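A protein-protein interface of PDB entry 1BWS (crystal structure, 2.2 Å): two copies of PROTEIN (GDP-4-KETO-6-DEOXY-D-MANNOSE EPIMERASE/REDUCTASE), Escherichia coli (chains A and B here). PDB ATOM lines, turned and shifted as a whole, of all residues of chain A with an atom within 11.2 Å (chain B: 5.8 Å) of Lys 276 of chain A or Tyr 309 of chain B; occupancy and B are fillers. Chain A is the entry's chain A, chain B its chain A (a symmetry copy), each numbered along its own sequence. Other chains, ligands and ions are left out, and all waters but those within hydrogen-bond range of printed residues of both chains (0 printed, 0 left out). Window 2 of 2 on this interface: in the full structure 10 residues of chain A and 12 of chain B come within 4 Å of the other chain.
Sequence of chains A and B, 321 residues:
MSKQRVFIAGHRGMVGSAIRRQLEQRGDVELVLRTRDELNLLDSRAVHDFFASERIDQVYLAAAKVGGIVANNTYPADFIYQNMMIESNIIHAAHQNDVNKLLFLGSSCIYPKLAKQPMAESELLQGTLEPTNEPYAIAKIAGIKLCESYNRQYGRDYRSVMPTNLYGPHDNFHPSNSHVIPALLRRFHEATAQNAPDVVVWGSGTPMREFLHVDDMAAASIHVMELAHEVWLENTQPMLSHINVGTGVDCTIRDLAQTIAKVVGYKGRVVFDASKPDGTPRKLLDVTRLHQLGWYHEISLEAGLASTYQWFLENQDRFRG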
ATOM      1  N   ARG A 187     -32.801 -14.627  -6.267  1.00  0.00           N
ATOM      2  CA  ARG A 187     -32.886 -13.575  -7.285  1.00  0.00           C
ATOM      3  C   ARG A 187     -34.323 -13.283  -7.807  1.00  0.00           C
ATOM      4  O   ARG A 187     -34.769 -12.117  -7.867  1.00  0.00           O
ATOM      5  CB  ARG A 187     -31.908 -13.828  -8.438  1.00  0.00           C
ATOM      6  CG  ARG A 187     -30.478 -14.009  -7.985  1.00  0.00           C
ATOM      7  CD  ARG A 187     -29.565 -14.143  -9.175  1.00  0.00           C
ATOM      8  NE  ARG A 187     -29.637 -12.950 -10.000  1.00  0.00           N
ATOM      9  CZ  ARG A 187     -29.225 -12.876 -11.262  1.00  0.00           C
ATOM     10  NH1 ARG A 187     -28.694 -13.934 -11.868  1.00  0.00           N
ATOM     11  NH2 ARG A 187     -29.323 -11.722 -11.905  1.00  0.00           N
ATOM     12  N   VAL A 200     -31.404 -11.044 -15.546  1.00  0.00           N
ATOM     13  CA  VAL A 200     -30.455 -11.558 -16.529  1.00  0.00           C
ATOM     14  C   VAL A 200     -29.581 -12.696 -15.978  1.00  0.00           C
ATOM     15  O   VAL A 200     -29.135 -12.614 -14.858  1.00  0.00           O
ATOM     16  CB  VAL A 200     -29.606 -10.420 -17.101  1.00  0.00           C
ATOM     17  CG1 VAL A 200     -28.391 -10.953 -17.939  1.00  0.00           C
ATOM     18  CG2 VAL A 200     -30.500  -9.453 -17.870  1.00  0.00           C
ATOM     19  N   VAL A 201     -29.454 -13.802 -16.722  1.00  0.00           N
ATOM     20  CA  VAL A 201     -28.637 -14.953 -16.341  1.00  0.00           C
ATOM     21  C   VAL A 201     -27.560 -15.078 -17.362  1.00  0.00           C
ATOM     22  O   VAL A 201     -27.872 -15.070 -18.552  1.00  0.00           O
ATOM     23  CB  VAL A 201     -29.452 -16.236 -16.386  1.00  0.00           C
ATOM     24  CG1 VAL A 201     -28.606 -17.417 -15.896  1.00  0.00           C
ATOM     25  CG2 VAL A 201     -30.708 -16.058 -15.514  1.00  0.00           C
ATOM     26  N   TRP A 202     -26.299 -15.075 -16.904  1.00  0.00           N
ATOM     27  CA  TRP A 202     -25.141 -15.182 -17.785  1.00  0.00           C
ATOM     28  C   TRP A 202     -25.279 -16.499 -18.536  1.00  0.00           C
ATOM     29  O   TRP A 202     -25.661 -17.498 -17.925  1.00  0.00           O
ATOM     30  CB  TRP A 202     -23.880 -15.344 -16.989  1.00  0.00           C
ATOM     31  CG  TRP A 202     -23.358 -14.193 -16.225  1.00  0.00           C
ATOM     32  CD1 TRP A 202     -22.523 -14.249 -15.125  1.00  0.00           C
ATOM     33  CD2 TRP A 202     -23.538 -12.811 -16.514  1.00  0.00           C
ATOM     34  NE1 TRP A 202     -22.112 -12.989 -14.772  1.00  0.00           N
ATOM     35  CE2 TRP A 202     -22.756 -12.079 -15.562  1.00  0.00           C
ATOM     36  CE3 TRP A 202     -24.282 -12.106 -17.477  1.00  0.00           C
ATOM     37  CZ2 TRP A 202     -22.626 -10.700 -15.604  1.00  0.00           C
ATOM     38  CZ3 TRP A 202     -24.149 -10.725 -17.522  1.00  0.00           C
ATOM     39  CH2 TRP A 202     -23.309 -10.036 -16.600  1.00  0.00           C
ATOM     40  N   GLY A 203     -24.937 -16.526 -19.826  1.00  0.00           N
ATOM     41  CA  GLY A 203     -24.972 -17.767 -20.581  1.00  0.00           C
ATOM     42  C   GLY A 203     -26.133 -17.916 -21.549  1.00  0.00           C
ATOM     43  O   GLY A 203     -27.103 -17.177 -21.485  1.00  0.00           O
ATOM     44  N   SER A 204     -25.992 -18.910 -22.429  1.00  0.00           N
ATOM     45  CA  SER A 204     -26.981 -19.289 -23.416  1.00  0.00           C
ATOM     46  C   SER A 204     -28.229 -19.988 -22.814  1.00  0.00           C
ATOM     47  O   SER A 204     -29.316 -19.964 -23.407  1.00  0.00           O
ATOM     48  CB  SER A 204     -26.331 -20.219 -24.470  1.00  0.00           C
ATOM     49  OG  SER A 204     -26.415 -21.593 -24.092  1.00  0.00           O
ATOM     50  N   GLY A 205     -28.055 -20.717 -21.717  1.00  0.00           N
ATOM     51  CA  GLY A 205     -29.169 -21.462 -21.117  1.00  0.00           C
ATOM     52  C   GLY A 205     -29.308 -22.879 -21.680  1.00  0.00           C
ATOM     53  O   GLY A 205     -30.206 -23.629 -21.287  1.00  0.00           O
ATOM     54  N   THR A 206     -28.442 -23.209 -22.636  1.00  0.00           N
ATOM     55  CA  THR A 206     -28.540 -24.472 -23.329  1.00  0.00           C
ATOM     56  C   THR A 206     -27.925 -25.643 -22.592  1.00  0.00           C
ATOM     57  O   THR A 206     -28.208 -26.787 -22.912  1.00  0.00           O
ATOM     58  CB  THR A 206     -27.864 -24.421 -24.717  1.00  0.00           C
ATOM     59  OG1 THR A 206     -26.485 -24.109 -24.557  1.00  0.00           O
ATOM     60  CG2 THR A 206     -28.492 -23.371 -25.591  1.00  0.00           C
ATOM     61  N   PRO A 207     -27.039 -25.386 -21.643  1.00  0.00           N
ATOM     62  CA  PRO A 207     -26.392 -26.518 -20.981  1.00  0.00           C
ATOM     63  C   PRO A 207     -27.333 -27.347 -20.125  1.00  0.00           C
ATOM     64  O   PRO A 207     -28.266 -26.808 -19.475  1.00  0.00           O
ATOM     65  CB  PRO A 207     -25.268 -25.871 -20.171  1.00  0.00           C
ATOM     66  CG  PRO A 207     -25.064 -24.490 -20.872  1.00  0.00           C
ATOM     67  CD  PRO A 207     -26.435 -24.099 -21.262  1.00  0.00           C
ATOM     68  N   ILE A 253     -30.566 -25.157 -18.210  1.00  0.00           N
ATOM     69  CA  ILE A 253     -30.610 -23.991 -17.314  1.00  0.00           C
ATOM     70  C   ILE A 253     -31.814 -23.097 -17.667  1.00  0.00           C
ATOM     71  O   ILE A 253     -32.526 -22.578 -16.765  1.00  0.00           O
ATOM     72  CB  ILE A 253     -29.282 -23.190 -17.392  1.00  0.00           C
ATOM     73  CG1 ILE A 253     -28.141 -24.077 -16.905  1.00  0.00           C
ATOM     74  CG2 ILE A 253     -29.312 -22.011 -16.465  1.00  0.00           C
ATOM     75  CD1 ILE A 253     -28.617 -25.118 -15.915  1.00  0.00           C
ATOM     76  N   VAL A 271     -34.059 -13.363 -19.062  1.00  0.00           N
ATOM     77  CA  VAL A 271     -33.162 -13.085 -20.181  1.00  0.00           C
ATOM     78  C   VAL A 271     -31.802 -13.797 -20.046  1.00  0.00           C
ATOM     79  O   VAL A 271     -31.193 -13.747 -18.986  1.00  0.00           O
ATOM     80  CB  VAL A 271     -32.861 -11.577 -20.171  1.00  0.00           C
ATOM     81  CG1 VAL A 271     -31.614 -11.277 -20.970  1.00  0.00           C
ATOM     82  CG2 VAL A 271     -34.062 -10.791 -20.662  1.00  0.00           C
ATOM     83  N   PHE A 272     -31.298 -14.388 -21.125  1.00  0.00           N
ATOM     84  CA  PHE A 272     -29.973 -15.007 -21.118  1.00  0.00           C
ATOM     85  C   PHE A 272     -28.920 -14.171 -21.841  1.00  0.00           C
ATOM     86  O   PHE A 272     -29.152 -13.775 -22.969  1.00  0.00           O
ATOM     87  CB  PHE A 272     -30.042 -16.413 -21.725  1.00  0.00           C
ATOM     88  CG  PHE A 272     -30.477 -17.452 -20.735  1.00  0.00           C
ATOM     89  CD1 PHE A 272     -31.839 -17.597 -20.422  1.00  0.00           C
ATOM     90  CD2 PHE A 272     -29.533 -18.132 -19.974  1.00  0.00           C
ATOM     91  CE1 PHE A 272     -32.289 -18.497 -19.430  1.00  0.00           C
ATOM     92  CE2 PHE A 272     -29.950 -19.045 -18.973  1.00  0.00           C
ATOM     93  CZ  PHE A 272     -31.337 -19.221 -18.689  1.00  0.00           C
ATOM     94  N   ASP A 273     -27.787 -13.876 -21.190  1.00  0.00           N
ATOM     95  CA  ASP A 273     -26.709 -13.127 -21.843  1.00  0.00           C
ATOM     96  C   ASP A 273     -25.707 -14.093 -22.467  1.00  0.00           C
ATOM     97  O   ASP A 273     -24.737 -14.539 -21.837  1.00  0.00           O
ATOM     98  CB  ASP A 273     -25.981 -12.165 -20.904  1.00  0.00           C
ATOM     99  CG  ASP A 273     -24.916 -11.334 -21.653  1.00  0.00           C
ATOM    100  OD1 ASP A 273     -24.521 -11.721 -22.805  1.00  0.00           O
ATOM    101  OD2 ASP A 273     -24.488 -10.287 -21.114  1.00  0.00           O
ATOM    102  N   ALA A 274     -25.936 -14.391 -23.731  1.00  0.00           N
ATOM    103  CA  ALA A 274     -25.127 -15.405 -24.328  1.00  0.00           C
ATOM    104  C   ALA A 274     -23.756 -14.920 -24.589  1.00  0.00           C
ATOM    105  O   ALA A 274     -22.920 -15.660 -25.136  1.00  0.00           O
ATOM    106  CB  ALA A 274     -25.781 -15.997 -25.575  1.00  0.00           C
ATOM    107  N   SER A 275     -23.520 -13.661 -24.252  1.00  0.00           N
ATOM    108  CA  SER A 275     -22.170 -13.173 -24.461  1.00  0.00           C
ATOM    109  C   SER A 275     -21.278 -13.804 -23.391  1.00  0.00           C
ATOM    110  O   SER A 275     -20.041 -13.762 -23.470  1.00  0.00           O
ATOM    111  CB  SER A 275     -22.077 -11.660 -24.465  1.00  0.00           C
ATOM    112  OG  SER A 275     -22.093 -11.117 -23.163  1.00  0.00           O
ATOM    113  N   LYS A 276     -21.912 -14.473 -22.436  1.00  0.00           N
ATOM    114  CA  LYS A 276     -21.135 -15.150 -21.412  1.00  0.00           C
ATOM    115  C   LYS A 276     -21.051 -16.630 -21.760  1.00  0.00           C
ATOM    116  O   LYS A 276     -22.016 -17.225 -22.260  1.00  0.00           O
ATOM    117  CB  LYS A 276     -21.706 -14.921 -20.012  1.00  0.00           C
ATOM    118  CG  LYS A 276     -22.084 -13.489 -19.754  1.00  0.00           C
ATOM    119  CD  LYS A 276     -20.851 -12.699 -19.858  1.00  0.00           C
ATOM    120  CE  LYS A 276     -20.955 -11.369 -19.148  1.00  0.00           C
ATOM    121  NZ  LYS A 276     -19.591 -10.813 -18.808  1.00  0.00           N
ATOM    122  N   PRO A 277     -19.862 -17.186 -21.536  1.00  0.00           N
ATOM    123  CA  PRO A 277     -19.560 -18.588 -21.824  1.00  0.00           C
ATOM    124  C   PRO A 277     -20.393 -19.593 -21.036  1.00  0.00           C
ATOM    125  O   PRO A 277     -20.898 -19.312 -19.937  1.00  0.00           O
ATOM    126  CB  PRO A 277     -18.093 -18.714 -21.395  1.00  0.00           C
ATOM    127  CG  PRO A 277     -17.953 -17.687 -20.255  1.00  0.00           C
ATOM    128  CD  PRO A 277     -18.754 -16.524 -20.812  1.00  0.00           C
ATOM    129  N   ASP A 278     -20.556 -20.765 -21.623  1.00  0.00           N
ATOM    130  CA  ASP A 278     -21.277 -21.831 -20.941  1.00  0.00           C
ATOM    131  C   ASP A 278     -20.223 -22.812 -20.454  1.00  0.00           C
ATOM    132  O   ASP A 278     -19.069 -22.746 -20.843  1.00  0.00           O
ATOM    133  CB  ASP A 278     -22.293 -22.554 -21.881  1.00  0.00           C
ATOM    134  CG  ASP A 278     -23.424 -21.649 -22.333  1.00  0.00           C
ATOM    135  OD1 ASP A 278     -23.963 -20.945 -21.474  1.00  0.00           O
ATOM    136  OD2 ASP A 278     -23.721 -21.577 -23.550  1.00  0.00           O
ATOM    137  N   GLY A 279     -20.626 -23.749 -19.624  1.00  0.00           N
ATOM    138  CA  GLY A 279     -19.699 -24.787 -19.175  1.00  0.00           C
ATOM    139  C   GLY A 279     -19.865 -25.938 -20.134  1.00  0.00           C
ATOM    140  O   GLY A 279     -20.213 -25.736 -21.298  1.00  0.00           O
ATOM    141  N   THR A 280     -19.653 -27.156 -19.681  1.00  0.00           N
ATOM    142  CA  THR A 280     -19.857 -28.227 -20.624  1.00  0.00           C
ATOM    143  C   THR A 280     -21.344 -28.293 -20.935  1.00  0.00           C
ATOM    144  O   THR A 280     -22.180 -27.828 -20.136  1.00  0.00           O
ATOM    145  CB  THR A 280     -19.299 -29.574 -20.119  1.00  0.00           C
ATOM    146  OG1 THR A 280     -19.841 -29.858 -18.826  1.00  0.00           O
ATOM    147  CG2 THR A 280     -17.778 -29.512 -20.055  1.00  0.00           C
ATOM    148  N   LEU B 185     -11.803  -5.700 -13.050  1.00  0.00           N
ATOM    149  CA  LEU B 185     -13.108  -5.849 -13.649  1.00  0.00           C
ATOM    150  C   LEU B 185     -12.862  -5.789 -15.149  1.00  0.00           C
ATOM    151  O   LEU B 185     -13.393  -6.606 -15.932  1.00  0.00           O
ATOM    152  CB  LEU B 185     -14.056  -4.724 -13.207  1.00  0.00           C
ATOM    153  CG  LEU B 185     -14.877  -5.050 -11.963  1.00  0.00           C
ATOM    154  CD1 LEU B 185     -15.496  -3.757 -11.325  1.00  0.00           C
ATOM    155  CD2 LEU B 185     -15.919  -6.120 -12.251  1.00  0.00           C
ATOM    156  N   HIS B 189     -13.307  -9.101 -17.738  1.00  0.00           N
ATOM    157  CA  HIS B 189     -14.284  -8.856 -18.780  1.00  0.00           C
ATOM    158  C   HIS B 189     -13.787  -9.227 -20.173  1.00  0.00           C
ATOM    159  O   HIS B 189     -14.483  -9.893 -20.953  1.00  0.00           O
ATOM    160  CB  HIS B 189     -14.565  -7.385 -18.820  1.00  0.00           C
ATOM    161  CG  HIS B 189     -15.516  -7.013 -19.910  1.00  0.00           C
ATOM    162  ND1 HIS B 189     -16.866  -7.293 -19.842  1.00  0.00           N
ATOM    163  CD2 HIS B 189     -15.315  -6.401 -21.102  1.00  0.00           C
ATOM    164  CE1 HIS B 189     -17.465  -6.818 -20.921  1.00  0.00           C
ATOM    165  NE2 HIS B 189     -16.538  -6.328 -21.726  1.00  0.00           N
ATOM    166  N   THR B 192     -13.043 -12.825 -20.481  1.00  0.00           N
ATOM    167  CA  THR B 192     -14.224 -13.627 -20.598  1.00  0.00           C
ATOM    168  C   THR B 192     -14.696 -13.588 -22.054  1.00  0.00           C
ATOM    169  O   THR B 192     -15.008 -14.618 -22.650  1.00  0.00           O
ATOM    170  CB  THR B 192     -15.253 -13.155 -19.626  1.00  0.00           C
ATOM    171  OG1 THR B 192     -14.763 -13.393 -18.298  1.00  0.00           O
ATOM    172  CG2 THR B 192     -16.551 -13.937 -19.826  1.00  0.00           C
ATOM    173  N   VAL B 263     -18.197 -12.688 -10.621  1.00  0.00           N
ATOM    174  CA  VAL B 263     -19.098 -11.603 -11.008  1.00  0.00           C
ATOM    175  C   VAL B 263     -19.181 -11.401 -12.567  1.00  0.00           C
ATOM    176  O   VAL B 263     -20.229 -11.148 -13.168  1.00  0.00           O
ATOM    177  CB  VAL B 263     -18.714 -10.254 -10.295  1.00  0.00           C
ATOM    178  CG1 VAL B 263     -19.384  -9.049 -11.008  1.00  0.00           C
ATOM    179  CG2 VAL B 263     -19.163 -10.307  -8.833  1.00  0.00           C
ATOM    180  N   VAL B 264     -18.063 -11.553 -13.238  1.00  0.00           N
ATOM    181  CA  VAL B 264     -18.057 -11.295 -14.639  1.00  0.00           C
ATOM    182  C   VAL B 264     -18.557 -12.447 -15.508  1.00  0.00           C
ATOM    183  O   VAL B 264     -18.876 -12.278 -16.690  1.00  0.00           O
ATOM    184  CB  VAL B 264     -16.696 -10.810 -15.010  1.00  0.00           C
ATOM    185  CG1 VAL B 264     -16.466 -10.934 -16.453  1.00  0.00           C
ATOM    186  CG2 VAL B 264     -16.582  -9.363 -14.553  1.00  0.00           C
ATOM    187  N   GLY B 265     -18.725 -13.605 -14.896  1.00  0.00           N
ATOM    188  CA  GLY B 265     -19.144 -14.771 -15.637  1.00  0.00           C
ATOM    189  C   GLY B 265     -17.937 -15.472 -16.328  1.00  0.00           C
ATOM    190  O   GLY B 265     -18.154 -16.254 -17.293  1.00  0.00           O
ATOM    191  N   GLY B 304     -21.828  -4.877  -4.324  1.00  0.00           N
ATOM    192  CA  GLY B 304     -21.207  -3.711  -4.915  1.00  0.00           C
ATOM    193  C   GLY B 304     -20.467  -4.037  -6.210  1.00  0.00           C
ATOM    194  O   GLY B 304     -20.462  -3.220  -7.149  1.00  0.00           O
ATOM    195  N   LEU B 305     -19.748  -5.165  -6.257  1.00  0.00           N
ATOM    196  CA  LEU B 305     -19.024  -5.438  -7.515  1.00  0.00           C
ATOM    197  C   LEU B 305     -19.984  -5.717  -8.718  1.00  0.00           C
ATOM    198  O   LEU B 305     -19.758  -5.302  -9.883  1.00  0.00           O
ATOM    199  CB  LEU B 305     -18.013  -6.583  -7.345  1.00  0.00           C
ATOM    200  CG  LEU B 305     -16.707  -6.508  -6.512  1.00  0.00           C
ATOM    201  CD1 LEU B 305     -16.112  -7.946  -6.316  1.00  0.00           C
ATOM    202  CD2 LEU B 305     -15.672  -5.598  -7.155  1.00  0.00           C
ATOM    203  N   ALA B 306     -21.050  -6.443  -8.417  1.00  0.00           N
ATOM    204  CA  ALA B 306     -22.053  -6.782  -9.403  1.00  0.00           C
ATOM    205  C   ALA B 306     -22.640  -5.529 -10.031  1.00  0.00           C
ATOM    206  O   ALA B 306     -22.745  -5.419 -11.240  1.00  0.00           O
ATOM    207  CB  ALA B 306     -23.145  -7.544  -8.736  1.00  0.00           C
ATOM    208  N   SER B 307     -23.113  -4.628  -9.196  1.00  0.00           N
ATOM    209  CA  SER B 307     -23.744  -3.392  -9.692  1.00  0.00           C
ATOM    210  C   SER B 307     -22.720  -2.489 -10.393  1.00  0.00           C
ATOM    211  O   SER B 307     -23.031  -1.772 -11.355  1.00  0.00           O
ATOM    212  CB  SER B 307     -24.326  -2.641  -8.499  1.00  0.00           C
ATOM    213  OG  SER B 307     -23.261  -2.053  -7.753  1.00  0.00           O
ATOM    214  N   THR B 308     -21.485  -2.523  -9.918  1.00  0.00           N
ATOM    215  CA  THR B 308     -20.424  -1.720 -10.517  1.00  0.00           C
ATOM    216  C   THR B 308     -20.100  -2.266 -11.918  1.00  0.00           C
ATOM    217  O   THR B 308     -19.925  -1.503 -12.862  1.00  0.00           O
ATOM    218  CB  THR B 308     -19.151  -1.705  -9.613  1.00  0.00           C
ATOM    219  OG1 THR B 308     -19.433  -1.090  -8.352  1.00  0.00           O
ATOM    220  CG2 THR B 308     -17.996  -0.980 -10.278  1.00  0.00           C
ATOM    221  N   TYR B 309     -20.053  -3.584 -12.075  1.00  0.00           N
ATOM    222  CA  TYR B 309     -19.810  -4.158 -13.406  1.00  0.00           C
ATOM    223  C   TYR B 309     -20.932  -3.752 -14.458  1.00  0.00           C
ATOM    224  O   TYR B 309     -20.675  -3.479 -15.620  1.00  0.00           O
ATOM    225  CB  TYR B 309     -19.598  -5.698 -13.286  1.00  0.00           C
ATOM    226  CG  TYR B 309     -19.369  -6.452 -14.603  1.00  0.00           C
ATOM    227  CD1 TYR B 309     -18.363  -6.079 -15.459  1.00  0.00           C
ATOM    228  CD2 TYR B 309     -20.164  -7.559 -14.956  1.00  0.00           C
ATOM    229  CE1 TYR B 309     -18.168  -6.730 -16.633  1.00  0.00           C
ATOM    230  CE2 TYR B 309     -20.010  -8.207 -16.171  1.00  0.00           C
ATOM    231  CZ  TYR B 309     -18.995  -7.788 -16.998  1.00  0.00           C
ATOM    232  OH  TYR B 309     -18.715  -8.459 -18.171  1.00  0.00           O
ATOM    233  N   GLN B 310     -22.177  -3.716 -14.027  1.00  0.00           N
ATOM    234  CA  GLN B 310     -23.290  -3.341 -14.900  1.00  0.00           C
ATOM    235  C   GLN B 310     -23.143  -1.895 -15.349  1.00  0.00           C
ATOM    236  O   GLN B 310     -23.401  -1.548 -16.498  1.00  0.00           O
ATOM    237  CB  GLN B 310     -24.623  -3.494 -14.156  1.00  0.00           C
ATOM    238  CG  GLN B 310     -25.813  -3.397 -15.085  1.00  0.00           C
ATOM    239  CD  GLN B 310     -25.892  -4.565 -16.045  1.00  0.00           C
ATOM    240  OE1 GLN B 310     -25.693  -5.720 -15.659  1.00  0.00           O
ATOM    241  NE2 GLN B 310     -26.171  -4.272 -17.311  1.00  0.00           N
ATOM    242  N   TRP B 311     -22.653  -1.051 -14.455  1.00  0.00           N
ATOM    243  CA  TRP B 311     -22.450   0.339 -14.822  1.00  0.00           C
ATOM    244  C   TRP B 311     -21.412   0.379 -15.912  1.00  0.00           C
ATOM    245  O   TRP B 311     -21.585   1.022 -16.925  1.00  0.00           O
ATOM    246  CB  TRP B 311     -22.021   1.186 -13.605  1.00  0.00           C
ATOM    247  CG  TRP B 311     -21.978   2.627 -13.905  1.00  0.00           C
ATOM    248  CD1 TRP B 311     -23.014   3.530 -13.814  1.00  0.00           C
ATOM    249  CD2 TRP B 311     -20.864   3.341 -14.421  1.00  0.00           C
ATOM    250  NE1 TRP B 311     -22.597   4.770 -14.279  1.00  0.00           N
ATOM    251  CE2 TRP B 311     -21.292   4.662 -14.686  1.00  0.00           C
ATOM    252  CE3 TRP B 311     -19.551   2.980 -14.732  1.00  0.00           C
ATOM    253  CZ2 TRP B 311     -20.457   5.610 -15.223  1.00  0.00           C
ATOM    254  CZ3 TRP B 311     -18.740   3.905 -15.296  1.00  0.00           C
ATOM    255  CH2 TRP B 311     -19.196   5.218 -15.537  1.00  0.00           C
ATOM    256  N   PHE B 312     -20.320  -0.331 -15.699  1.00  0.00           N
ATOM    257  CA  PHE B 312     -19.282  -0.408 -16.712  1.00  0.00           C
ATOM    258  C   PHE B 312     -19.867  -0.927 -18.022  1.00  0.00           C
ATOM    259  O   PHE B 312     -19.491  -0.473 -19.121  1.00  0.00           O
ATOM    260  CB  PHE B 312     -18.151  -1.334 -16.229  1.00  0.00           C
ATOM    261  CG  PHE B 312     -17.235  -1.787 -17.320  1.00  0.00           C
ATOM    262  CD1 PHE B 312     -16.224  -0.958 -17.766  1.00  0.00           C
ATOM    263  CD2 PHE B 312     -17.438  -3.030 -17.946  1.00  0.00           C
ATOM    264  CE1 PHE B 312     -15.399  -1.349 -18.820  1.00  0.00           C
ATOM    265  CE2 PHE B 312     -16.660  -3.415 -19.003  1.00  0.00           C
ATOM    266  CZ  PHE B 312     -15.610  -2.587 -19.434  1.00  0.00           C
ATOM    267  N   LEU B 313     -20.739  -1.920 -17.913  1.00  0.00           N
ATOM    268  CA  LEU B 313     -21.384  -2.489 -19.107  1.00  0.00           C
ATOM    269  C   LEU B 313     -22.229  -1.401 -19.746  1.00  0.00           C
ATOM    270  O   LEU B 313     -22.163  -1.206 -20.955  1.00  0.00           O
ATOM    271  CB  LEU B 313     -22.289  -3.703 -18.803  1.00  0.00           C
ATOM    272  CG  LEU B 313     -21.575  -4.981 -18.400  1.00  0.00           C
ATOM    273  CD1 LEU B 313     -22.624  -6.025 -18.381  1.00  0.00           C
ATOM    274  CD2 LEU B 313     -20.509  -5.281 -19.385  1.00  0.00           C
ATOM    275  N   GLU B 314     -23.011  -0.677 -18.941  1.00  0.00           N
ATOM    276  CA  GLU B 314     -23.829   0.405 -19.504  1.00  0.00           C
ATOM    277  C   GLU B 314     -23.050   1.637 -19.962  1.00  0.00           C
ATOM    278  O   GLU B 314     -23.619   2.533 -20.550  1.00  0.00           O
ATOM    279  CB  GLU B 314     -24.969   0.776 -18.577  1.00  0.00           C
ATOM    280  CG  GLU B 314     -25.795  -0.439 -18.267  1.00  0.00           C
ATOM    281  CD  GLU B 314     -26.814  -0.263 -17.157  1.00  0.00           C
ATOM    282  OE1 GLU B 314     -27.041   0.893 -16.759  1.00  0.00           O
ATOM    283  OE2 GLU B 314     -27.424  -1.287 -16.736  1.00  0.00           O
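The indole nitrogen (NE1) of Trp 202 of chain A lies within hydrogen-bond range of the backbone carbonyl oxygen (O) of Val 263 of chain B.
OH of Tyr 309 of chain B sits at hydrogen-bond distance from NZ of Lys 276 of chain A, 2.6 Å away.
The backbone carbonyl oxygen of Val 264 of chain B lies within hydrogen-bond range of the side-chain amino group of Lys 276 of chain A, at 2.7 Å.
N of Gly 265 of chain B lies close to NE1 of Trp 202 of chain A.
ND1 of His 189 of chain B sits at hydrogen-bond distance from OH of Tyr 309 of chain B (2.8 Å).
Trp 202 of chain A touches Val 264 of chain B.
Trp 202 of chain A touches Tyr 309 of chain B.
CD of Pro 277 of chain A touches CG2 of Thr 192 of chain B, 3.5 Å away.
CG of Pro 277 of chain A touches O of Gly 265 of chain B, at 3.3 Å.
Of chain B, only Val 264 (2.7 Å) and Tyr 309 (2.6 Å) come within 4 Å of Lys 276 of chain A.
Tyr 309 of chain B touches two residues of chain A.
No residue of chain A comes within 4 Å of His 189 of chain B.
Val 263 of chain B touches just one residue of chain A: Trp 202.
Of chain A, only Trp 202 (3.7 Å) and Lys 276 (2.7 Å) come within 4 Å of Val 264 of chain B.
Of the printed residues of chain A, Gly 265 of chain B touches Trp 202 (3.4 Å) and Pro 277 (3.3 Å).
No residue of chain A comes within 4 Å of Ser 307 of chain B.
Thr 308 of chain B touches none of the printed residues of chain A.
No residue of chain A comes within 4 Å of Gln 310 of chain B.
No residue of chain A comes within 4 Å of Phe 312 of chain B.
No residue of chain A comes within 4 Å of Leu 313 of chain B.
Of the printed residues of chain B, Pro 277 of chain A touches Thr 192 (3.5 Å) and Gly 265 (3.3 Å).
Printed residues of chain B within 4 Å of Trp 202 of chain A: Val 263, Val 264, Gly 265 and Tyr 309.
Val 200 of chain A touches none of the printed residues of chain B.
The nearest residue of chain B that does not touch Lys 276 of chain A is Thr 192 of chain B (4.5 Å).
The nearest residue of chain A that does not touch Tyr 309 of chain B is Ser 275 of chain A (6.6 Å).
The nearest printed residue of chain B that does not touch Trp 202 of chain A is Leu 313 of chain B (4.4 Å).
Of the 17 printed residues of chain B, 5 touch a printed residue of chain A.
Printed residues of chain A that touch a printed residue of chain B: Trp 202, Lys 276 and Pro 277.
Hydrophobic or aromatic side chains of chain A within 4 Å of the printed part of chain B: Trp 202 and Pro 277.
Among the printed residues, 8 pairs touch across the chains.
No position is printed for both chains.
Of the 8 pairs that touch across the chains among the printed residues, none has its exchanged pair printed and touching as well.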
